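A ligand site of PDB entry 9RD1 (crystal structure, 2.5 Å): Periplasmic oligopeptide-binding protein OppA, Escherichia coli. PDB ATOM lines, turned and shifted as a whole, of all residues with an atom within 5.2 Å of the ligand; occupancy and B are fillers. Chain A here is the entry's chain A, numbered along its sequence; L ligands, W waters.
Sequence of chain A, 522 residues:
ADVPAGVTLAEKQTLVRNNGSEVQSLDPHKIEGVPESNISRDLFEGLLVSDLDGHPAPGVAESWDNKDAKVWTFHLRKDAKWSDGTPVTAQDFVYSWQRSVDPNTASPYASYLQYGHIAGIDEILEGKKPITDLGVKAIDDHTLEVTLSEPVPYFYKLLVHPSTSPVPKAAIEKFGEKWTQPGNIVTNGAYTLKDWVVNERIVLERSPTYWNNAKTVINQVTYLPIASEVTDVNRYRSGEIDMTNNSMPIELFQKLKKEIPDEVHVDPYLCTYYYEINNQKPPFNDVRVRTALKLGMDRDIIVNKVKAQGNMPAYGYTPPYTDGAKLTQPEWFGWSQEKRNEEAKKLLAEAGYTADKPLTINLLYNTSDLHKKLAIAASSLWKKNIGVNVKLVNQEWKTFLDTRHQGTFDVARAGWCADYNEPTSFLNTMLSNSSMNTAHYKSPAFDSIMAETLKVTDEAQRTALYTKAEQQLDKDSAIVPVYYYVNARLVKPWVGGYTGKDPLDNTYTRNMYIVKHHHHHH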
ATOM      1  N   GLY A  20      27.405  -7.706  26.669  1.00  0.00           N
ATOM      2  CA  GLY A  20      26.002  -7.247  26.671  1.00  0.00           C
ATOM      3  C   GLY A  20      25.124  -8.030  27.624  1.00  0.00           C
ATOM      4  O   GLY A  20      24.056  -7.515  28.001  1.00  0.00           O
ATOM      5  N   SER A  21      25.546  -9.244  28.015  1.00  0.00           N
ATOM      6  CA  SER A  21      24.764 -10.159  28.886  1.00  0.00           C
ATOM      7  C   SER A  21      25.615 -11.356  29.308  1.00  0.00           C
ATOM      8  O   SER A  21      26.707 -11.551  28.746  1.00  0.00           O
ATOM      9  CB  SER A  21      23.502 -10.611  28.188  1.00  0.00           C
ATOM     10  OG  SER A  21      23.788 -11.124  26.897  1.00  0.00           O
ATOM     11  N   GLU A  32      23.151 -19.803  20.929  1.00  0.00           N
ATOM     12  CA  GLU A  32      22.416 -19.307  19.732  1.00  0.00           C
ATOM     13  C   GLU A  32      22.516 -17.773  19.665  1.00  0.00           C
ATOM     14  O   GLU A  32      22.128 -17.213  18.624  1.00  0.00           O
ATOM     15  CB  GLU A  32      20.941 -19.709  19.808  1.00  0.00           C
ATOM     16  CG  GLU A  32      20.220 -19.126  21.012  1.00  0.00           C
ATOM     17  CD  GLU A  32      18.892 -19.799  21.338  1.00  0.00           C
ATOM     18  OE1 GLU A  32      18.737 -20.245  22.484  1.00  0.00           O
ATOM     19  OE2 GLU A  32      18.043 -19.880  20.446  1.00  0.00           O
ATOM     20  N   GLY A  33      23.047 -17.139  20.713  1.00  0.00           N
ATOM     21  CA  GLY A  33      23.132 -15.676  20.770  1.00  0.00           C
ATOM     22  C   GLY A  33      24.475 -15.118  20.311  1.00  0.00           C
ATOM     23  O   GLY A  33      25.471 -15.858  20.362  1.00  0.00           O
ATOM     24  N   VAL A  34      24.471 -13.844  19.916  1.00  0.00           N
ATOM     25  CA  VAL A  34      25.688 -13.130  19.433  1.00  0.00           C
ATOM     26  C   VAL A  34      26.716 -13.072  20.569  1.00  0.00           C
ATOM     27  O   VAL A  34      27.899 -13.350  20.300  1.00  0.00           O
ATOM     28  CB  VAL A  34      25.332 -11.718  18.934  1.00  0.00           C
ATOM     29  CG1 VAL A  34      26.570 -10.877  18.660  1.00  0.00           C
ATOM     30  CG2 VAL A  34      24.432 -11.764  17.717  1.00  0.00           C
ATOM     31  N   PRO A  35      26.328 -12.717  21.814  1.00  0.00           N
ATOM     32  CA  PRO A  35      27.278 -12.657  22.937  1.00  0.00           C
ATOM     33  C   PRO A  35      28.031 -13.984  23.088  1.00  0.00           C
ATOM     34  O   PRO A  35      29.232 -13.954  23.253  1.00  0.00           O
ATOM     35  CB  PRO A  35      26.379 -12.435  24.155  1.00  0.00           C
ATOM     36  CG  PRO A  35      25.129 -11.798  23.603  1.00  0.00           C
ATOM     37  CD  PRO A  35      24.966 -12.354  22.202  1.00  0.00           C
ATOM     38  N   TYR A 109      21.065 -24.715  17.826  1.00  0.00           N
ATOM     39  CA  TYR A 109      21.649 -24.629  16.464  1.00  0.00           C
ATOM     40  C   TYR A 109      21.801 -26.039  15.869  1.00  0.00           C
ATOM     41  O   TYR A 109      22.708 -26.252  15.032  1.00  0.00           O
ATOM     42  CB  TYR A 109      22.984 -23.863  16.522  1.00  0.00           C
ATOM     43  CG  TYR A 109      22.871 -22.449  16.016  1.00  0.00           C
ATOM     44  CD1 TYR A 109      23.438 -22.073  14.808  1.00  0.00           C
ATOM     45  CD2 TYR A 109      22.154 -21.494  16.724  1.00  0.00           C
ATOM     46  CE1 TYR A 109      23.323 -20.777  14.327  1.00  0.00           C
ATOM     47  CE2 TYR A 109      22.020 -20.194  16.258  1.00  0.00           C
ATOM     48  CZ  TYR A 109      22.615 -19.833  15.062  1.00  0.00           C
ATOM     49  OH  TYR A 109      22.498 -18.559  14.591  1.00  0.00           O
ATOM     50  N   HIS A 161      30.818 -20.198  11.676  1.00  0.00           N
ATOM     51  CA  HIS A 161      29.914 -20.097  12.857  1.00  0.00           C
ATOM     52  C   HIS A 161      30.392 -21.017  13.971  1.00  0.00           C
ATOM     53  O   HIS A 161      30.718 -22.172  13.728  1.00  0.00           O
ATOM     54  CB  HIS A 161      28.460 -20.387  12.461  1.00  0.00           C
ATOM     55  CG  HIS A 161      27.491 -19.977  13.520  1.00  0.00           C
ATOM     56  ND1 HIS A 161      26.967 -20.879  14.422  1.00  0.00           N
ATOM     57  CD2 HIS A 161      26.998 -18.763  13.857  1.00  0.00           C
ATOM     58  CE1 HIS A 161      26.168 -20.241  15.256  1.00  0.00           C
ATOM     59  NE2 HIS A 161      26.166 -18.954  14.933  1.00  0.00           N
ATOM     60  N   ASN A 245      29.691  -2.859  24.005  1.00  0.00           N
ATOM     61  CA  ASN A 245      28.760  -3.689  23.197  1.00  0.00           C
ATOM     62  C   ASN A 245      28.202  -2.782  22.091  1.00  0.00           C
ATOM     63  O   ASN A 245      28.176  -1.552  22.296  1.00  0.00           O
ATOM     64  CB  ASN A 245      27.653  -4.304  24.059  1.00  0.00           C
ATOM     65  CG  ASN A 245      26.814  -5.326  23.312  1.00  0.00           C
ATOM     66  OD1 ASN A 245      27.284  -5.954  22.362  1.00  0.00           O
ATOM     67  ND2 ASN A 245      25.576  -5.507  23.734  1.00  0.00           N
ATOM     68  N   SER A 247      25.314  -2.071  21.269  1.00  0.00           N
ATOM     69  CA  SER A 247      23.968  -1.556  21.641  1.00  0.00           C
ATOM     70  C   SER A 247      24.171  -0.183  22.293  1.00  0.00           C
ATOM     71  O   SER A 247      24.758  -0.135  23.400  1.00  0.00           O
ATOM     72  CB  SER A 247      23.238  -2.513  22.550  1.00  0.00           C
ATOM     73  OG  SER A 247      21.903  -2.083  22.770  1.00  0.00           O
ATOM     74  N   ASN A 366      14.384  -8.610  26.710  1.00  0.00           N
ATOM     75  CA  ASN A 366      15.564  -8.935  27.552  1.00  0.00           C
ATOM     76  C   ASN A 366      16.104  -7.645  28.170  1.00  0.00           C
ATOM     77  O   ASN A 366      16.141  -6.623  27.442  1.00  0.00           O
ATOM     78  CB  ASN A 366      16.666  -9.664  26.764  1.00  0.00           C
ATOM     79  CG  ASN A 366      17.095  -8.915  25.526  1.00  0.00           C
ATOM     80  OD1 ASN A 366      16.262  -8.512  24.718  1.00  0.00           O
ATOM     81  ND2 ASN A 366      18.389  -8.737  25.347  1.00  0.00           N
ATOM     82  N   HIS A 371      15.972  -1.499  24.745  1.00  0.00           N
ATOM     83  CA  HIS A 371      14.791  -2.385  24.550  1.00  0.00           C
ATOM     84  C   HIS A 371      13.612  -1.892  25.396  1.00  0.00           C
ATOM     85  O   HIS A 371      12.474  -1.960  24.894  1.00  0.00           O
ATOM     86  CB  HIS A 371      15.149  -3.855  24.840  1.00  0.00           C
ATOM     87  CG  HIS A 371      16.189  -4.420  23.942  1.00  0.00           C
ATOM     88  ND1 HIS A 371      16.346  -3.997  22.639  1.00  0.00           N
ATOM     89  CD2 HIS A 371      17.123  -5.373  24.151  1.00  0.00           C
ATOM     90  CE1 HIS A 371      17.333  -4.668  22.077  1.00  0.00           C
ATOM     91  NE2 HIS A 371      17.829  -5.517  22.984  1.00  0.00           N
ATOM     92  N   TRP A 397      18.843 -12.442  29.925  1.00  0.00           N
ATOM     93  CA  TRP A 397      19.138 -12.910  28.542  1.00  0.00           C
ATOM     94  C   TRP A 397      18.894 -14.415  28.387  1.00  0.00           C
ATOM     95  O   TRP A 397      18.311 -14.815  27.364  1.00  0.00           O
ATOM     96  CB  TRP A 397      20.569 -12.516  28.166  1.00  0.00           C
ATOM     97  CG  TRP A 397      21.051 -13.089  26.866  1.00  0.00           C
ATOM     98  CD1 TRP A 397      22.008 -14.044  26.699  1.00  0.00           C
ATOM     99  CD2 TRP A 397      20.591 -12.746  25.553  1.00  0.00           C
ATOM    100  NE1 TRP A 397      22.173 -14.323  25.367  1.00  0.00           N
ATOM    101  CE2 TRP A 397      21.319 -13.538  24.636  1.00  0.00           C
ATOM    102  CE3 TRP A 397      19.628 -11.850  25.050  1.00  0.00           C
ATOM    103  CZ2 TRP A 397      21.126 -13.461  23.265  1.00  0.00           C
ATOM    104  CZ3 TRP A 397      19.440 -11.783  23.687  1.00  0.00           C
ATOM    105  CH2 TRP A 397      20.178 -12.577  22.809  1.00  0.00           C
ATOM    106  N   LEU A 401      15.568 -16.180  26.191  1.00  0.00           N
ATOM    107  CA  LEU A 401      15.774 -17.116  25.042  1.00  0.00           C
ATOM    108  C   LEU A 401      15.021 -18.429  25.288  1.00  0.00           C
ATOM    109  O   LEU A 401      14.397 -18.931  24.330  1.00  0.00           O
ATOM    110  CB  LEU A 401      17.268 -17.359  24.824  1.00  0.00           C
ATOM    111  CG  LEU A 401      18.070 -16.167  24.302  1.00  0.00           C
ATOM    112  CD1 LEU A 401      19.542 -16.530  24.165  1.00  0.00           C
ATOM    113  CD2 LEU A 401      17.516 -15.660  22.979  1.00  0.00           C
ATOM    114  N   ARG A 404      11.124 -18.058  24.897  1.00  0.00           N
ATOM    115  CA  ARG A 404      10.737 -17.942  23.472  1.00  0.00           C
ATOM    116  C   ARG A 404      10.699 -19.334  22.821  1.00  0.00           C
ATOM    117  O   ARG A 404       9.797 -19.564  22.017  1.00  0.00           O
ATOM    118  CB  ARG A 404      11.677 -16.990  22.729  1.00  0.00           C
ATOM    119  CG  ARG A 404      11.511 -15.530  23.135  1.00  0.00           C
ATOM    120  CD  ARG A 404      12.661 -14.675  22.635  1.00  0.00           C
ATOM    121  NE  ARG A 404      12.630 -14.524  21.177  1.00  0.00           N
ATOM    122  CZ  ARG A 404      13.669 -14.179  20.420  1.00  0.00           C
ATOM    123  NH1 ARG A 404      14.853 -13.947  20.960  1.00  0.00           N
ATOM    124  NH2 ARG A 404      13.513 -14.068  19.114  1.00  0.00           N
ATOM    125  N   ARG A 413      10.242  -8.753  21.871  1.00  0.00           N
ATOM    126  CA  ARG A 413      11.324  -7.961  21.220  1.00  0.00           C
ATOM    127  C   ARG A 413      12.337  -8.970  20.665  1.00  0.00           C
ATOM    128  O   ARG A 413      12.811  -9.800  21.454  1.00  0.00           O
ATOM    129  CB  ARG A 413      11.956  -6.983  22.221  1.00  0.00           C
ATOM    130  CG  ARG A 413      13.251  -6.352  21.736  1.00  0.00           C
ATOM    131  CD  ARG A 413      14.488  -7.177  22.085  1.00  0.00           C
ATOM    132  NE  ARG A 413      15.442  -7.233  20.997  1.00  0.00           N
ATOM    133  CZ  ARG A 413      16.558  -7.955  20.989  1.00  0.00           C
ATOM    134  NH1 ARG A 413      16.877  -8.711  22.036  1.00  0.00           N
ATOM    135  NH2 ARG A 413      17.351  -7.934  19.944  1.00  0.00           N
ATOM    136  N   GLY A 415      15.639  -9.856  17.515  1.00  0.00           N
ATOM    137  CA  GLY A 415      16.770  -9.356  16.703  1.00  0.00           C
ATOM    138  C   GLY A 415      17.593 -10.524  16.186  1.00  0.00           C
ATOM    139  O   GLY A 415      18.250 -11.185  17.012  1.00  0.00           O
ATOM    140  N   TRP A 416      17.543 -10.780  14.876  1.00  0.00           N
ATOM    141  CA  TRP A 416      18.333 -11.845  14.207  1.00  0.00           C
ATOM    142  C   TRP A 416      19.509 -11.235  13.452  1.00  0.00           C
ATOM    143  O   TRP A 416      19.270 -10.300  12.662  1.00  0.00           O
ATOM    144  CB  TRP A 416      17.460 -12.686  13.261  1.00  0.00           C
ATOM    145  CG  TRP A 416      18.143 -13.946  12.855  1.00  0.00           C
ATOM    146  CD1 TRP A 416      18.674 -14.256  11.640  1.00  0.00           C
ATOM    147  CD2 TRP A 416      18.439 -15.060  13.714  1.00  0.00           C
ATOM    148  NE1 TRP A 416      19.258 -15.499  11.670  1.00  0.00           N
ATOM    149  CE2 TRP A 416      19.128 -16.014  12.931  1.00  0.00           C
ATOM    150  CE3 TRP A 416      18.177 -15.350  15.060  1.00  0.00           C
ATOM    151  CZ2 TRP A 416      19.550 -17.234  13.455  1.00  0.00           C
ATOM    152  CZ3 TRP A 416      18.604 -16.557  15.573  1.00  0.00           C
ATOM    153  CH2 TRP A 416      19.273 -17.484  14.786  1.00  0.00           C
ATOM    154  N   CYS A 417      20.725 -11.741  13.698  1.00  0.00           N
ATOM    155  CA  CYS A 417      21.961 -11.407  12.944  1.00  0.00           C
ATOM    156  C   CYS A 417      22.344 -12.597  12.058  1.00  0.00           C
ATOM    157  O   CYS A 417      22.333 -13.741  12.557  1.00  0.00           O
ATOM    158  CB  CYS A 417      23.108 -11.066  13.891  1.00  0.00           C
ATOM    159  SG  CYS A 417      22.954  -9.437  14.663  1.00  0.00           S
ATOM    160  N   ALA A 418      22.640 -12.337  10.775  1.00  0.00           N
ATOM    161  CA  ALA A 418      23.106 -13.337   9.796  1.00  0.00           C
ATOM    162  C   ALA A 418      24.322 -14.068  10.361  1.00  0.00           C
ATOM    163  O   ALA A 418      25.224 -13.390  10.890  1.00  0.00           O
ATOM    164  CB  ALA A 418      23.424 -12.671   8.478  1.00  0.00           C
ATOM    165  N   ASP A 419      24.329 -15.399  10.269  1.00  0.00           N
ATOM    166  CA  ASP A 419      25.478 -16.281  10.625  1.00  0.00           C
ATOM    167  C   ASP A 419      26.449 -16.321   9.442  1.00  0.00           C
ATOM    168  O   ASP A 419      27.663 -16.462   9.677  1.00  0.00           O
ATOM    169  CB  ASP A 419      24.994 -17.683  11.008  1.00  0.00           C
ATOM    170  CG  ASP A 419      24.039 -17.701  12.185  1.00  0.00           C
ATOM    171  OD1 ASP A 419      24.364 -17.077  13.210  1.00  0.00           O
ATOM    172  OD2 ASP A 419      22.967 -18.326  12.060  1.00  0.00           O
ATOM    173  N   TYR A 485      19.434  -3.083  11.705  1.00  0.00           N
ATOM    174  CA  TYR A 485      20.502  -2.658  12.644  1.00  0.00           C
ATOM    175  C   TYR A 485      21.587  -1.857  11.920  1.00  0.00           C
ATOM    176  O   TYR A 485      21.686  -1.915  10.678  1.00  0.00           O
ATOM    177  CB  TYR A 485      21.193  -3.871  13.279  1.00  0.00           C
ATOM    178  CG  TYR A 485      20.562  -4.425  14.535  1.00  0.00           C
ATOM    179  CD1 TYR A 485      19.386  -5.149  14.481  1.00  0.00           C
ATOM    180  CD2 TYR A 485      21.175  -4.260  15.766  1.00  0.00           C
ATOM    181  CE1 TYR A 485      18.821  -5.684  15.630  1.00  0.00           C
ATOM    182  CE2 TYR A 485      20.619  -4.783  16.923  1.00  0.00           C
ATOM    183  CZ  TYR A 485      19.438  -5.497  16.861  1.00  0.00           C
ATOM    184  OH  TYR A 485      18.884  -6.006  17.997  1.00  0.00           O
HETATM  185  N1  LIG L   1      22.538 -15.497  14.681  1.00  0.00           N
HETATM  186  C1  LIG L   1      22.615 -15.448  16.127  1.00  0.00           C
HETATM  187  C2  LIG L   1      21.569 -14.523  16.614  1.00  0.00           C
HETATM  188  O1  LIG L   1      21.161 -13.615  15.936  1.00  0.00           O
HETATM  189  N2  LIG L   1      21.112 -14.815  17.800  1.00  0.00           N
HETATM  190  C3  LIG L   1      20.173 -14.004  18.522  1.00  0.00           C
HETATM  191  C4  LIG L   1      21.059 -12.908  19.098  1.00  0.00           C
HETATM  192  O2  LIG L   1      21.977 -13.182  19.789  1.00  0.00           O
HETATM  193  C5  LIG L   1      19.509 -14.770  19.641  1.00  0.00           C
HETATM  194  O3  LIG L   1      18.209 -15.231  19.281  1.00  0.00           O
HETATM  195  N3  LIG L   1      22.188  -9.047  23.921  1.00  0.00           N
HETATM  196  C6  LIG L   1      21.869  -8.499  22.606  1.00  0.00           C
HETATM  197  C7  LIG L   1      20.639  -7.590  22.631  1.00  0.00           C
HETATM  198  O4  LIG L   1      19.613  -7.986  23.145  1.00  0.00           O
HETATM  199  C8  LIG L   1      21.784  -9.597  21.559  1.00  0.00           C
HETATM  200  C9  LIG L   1      20.406  -9.772  20.986  1.00  0.00           C
HETATM  201  C10 LIG L   1      20.455  -9.545  19.513  1.00  0.00           C
HETATM  202  C11 LIG L   1      21.468 -10.467  18.932  1.00  0.00           C
HETATM  203  N4  LIG L   1      20.811 -11.709  18.613  1.00  0.00           N
HETATM  204  O5  LIG L   1      20.770  -6.460  22.174  1.00  0.00           O
HETATM  205  O   HOH W   1      21.923  -7.178  26.308  1.00  0.00           O
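The backbone carbonyl oxygen (O) of Cys 417 is in hydrogen-bond range of a nitrogen (N1) of the ligand, 2.8 Å away. N of Cys 417 sits at hydrogen-bond distance from O1 of the ligand (3.0 Å). O4 of the ligand sits at hydrogen-bond distance from NE2 of His 371, 3.1 Å away. The backbone carbonyl oxygen of Gly 415 is in hydrogen-bond range of a nitrogen (N4) of the ligand, at 3.1 Å. An oxygen (O2) of the ligand lies within hydrogen-bond range of the backbone NH of Val 34 (2.6 Å). O of Glu 32 is in hydrogen-bond range of N2 of the ligand, 2.7 Å away. OH of Tyr 109 is in hydrogen-bond range of N1 of the ligand (3.1 Å). NH1 of Arg 413 is in salt-bridge range of O4 of the ligand (3.0 Å). The side-chain carboxylate (OD1) of Asp 419 lies within salt-bridge range of a nitrogen (N1) of the ligand (2.8 Å). ND2 of Asn 366 lies within hydrogen-bond range of O4 of the ligand (2.6 Å).
Water W1 bridges the backbone carbonyl oxygen (O) of Gly 20 (2.7 Å) and a nitrogen (N3) of the ligand (3.0 Å).
The side-chain carboxylate of Asp 419 sits at hydrogen-bond distance from the side-chain hydroxyl of Tyr 109 (2.6 Å). NE2 of His 161 lies within hydrogen-bond range of OD1 of Asp 419 (3.1 Å). The guanidinium group (NH2) of Arg 413 is in hydrogen-bond range of the side-chain hydroxyl (OH) of Tyr 485. NH1 of Arg 413 lies close to NE2 of His 371. The side-chain amide oxygen (OD1) of Asn 366 sits at hydrogen-bond distance from the guanidinium group (NH1) of Arg 413 (2.8 Å).
Ser 21 touches the ligand (OG to N3, 3.97 Å). Gly 33 touches the ligand. CD of Pro 35 touches O2 of the ligand, at 3.9 Å. CH2 of Trp 397 touches C9 of the ligand (3.4 Å). Leu 401 touches the ligand (CD2 to O3, 3.8 Å). NH1 of Arg 404 touches O3 of the ligand, at 3.97 Å. CE3 of Trp 416 touches O1 of the ligand, at 3.6 Å. Of the 22 residues printed, 16 come within 4 Å of the ligand. The nearest printed residue that does not touch the ligand is Tyr 485 (4.2 Å).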
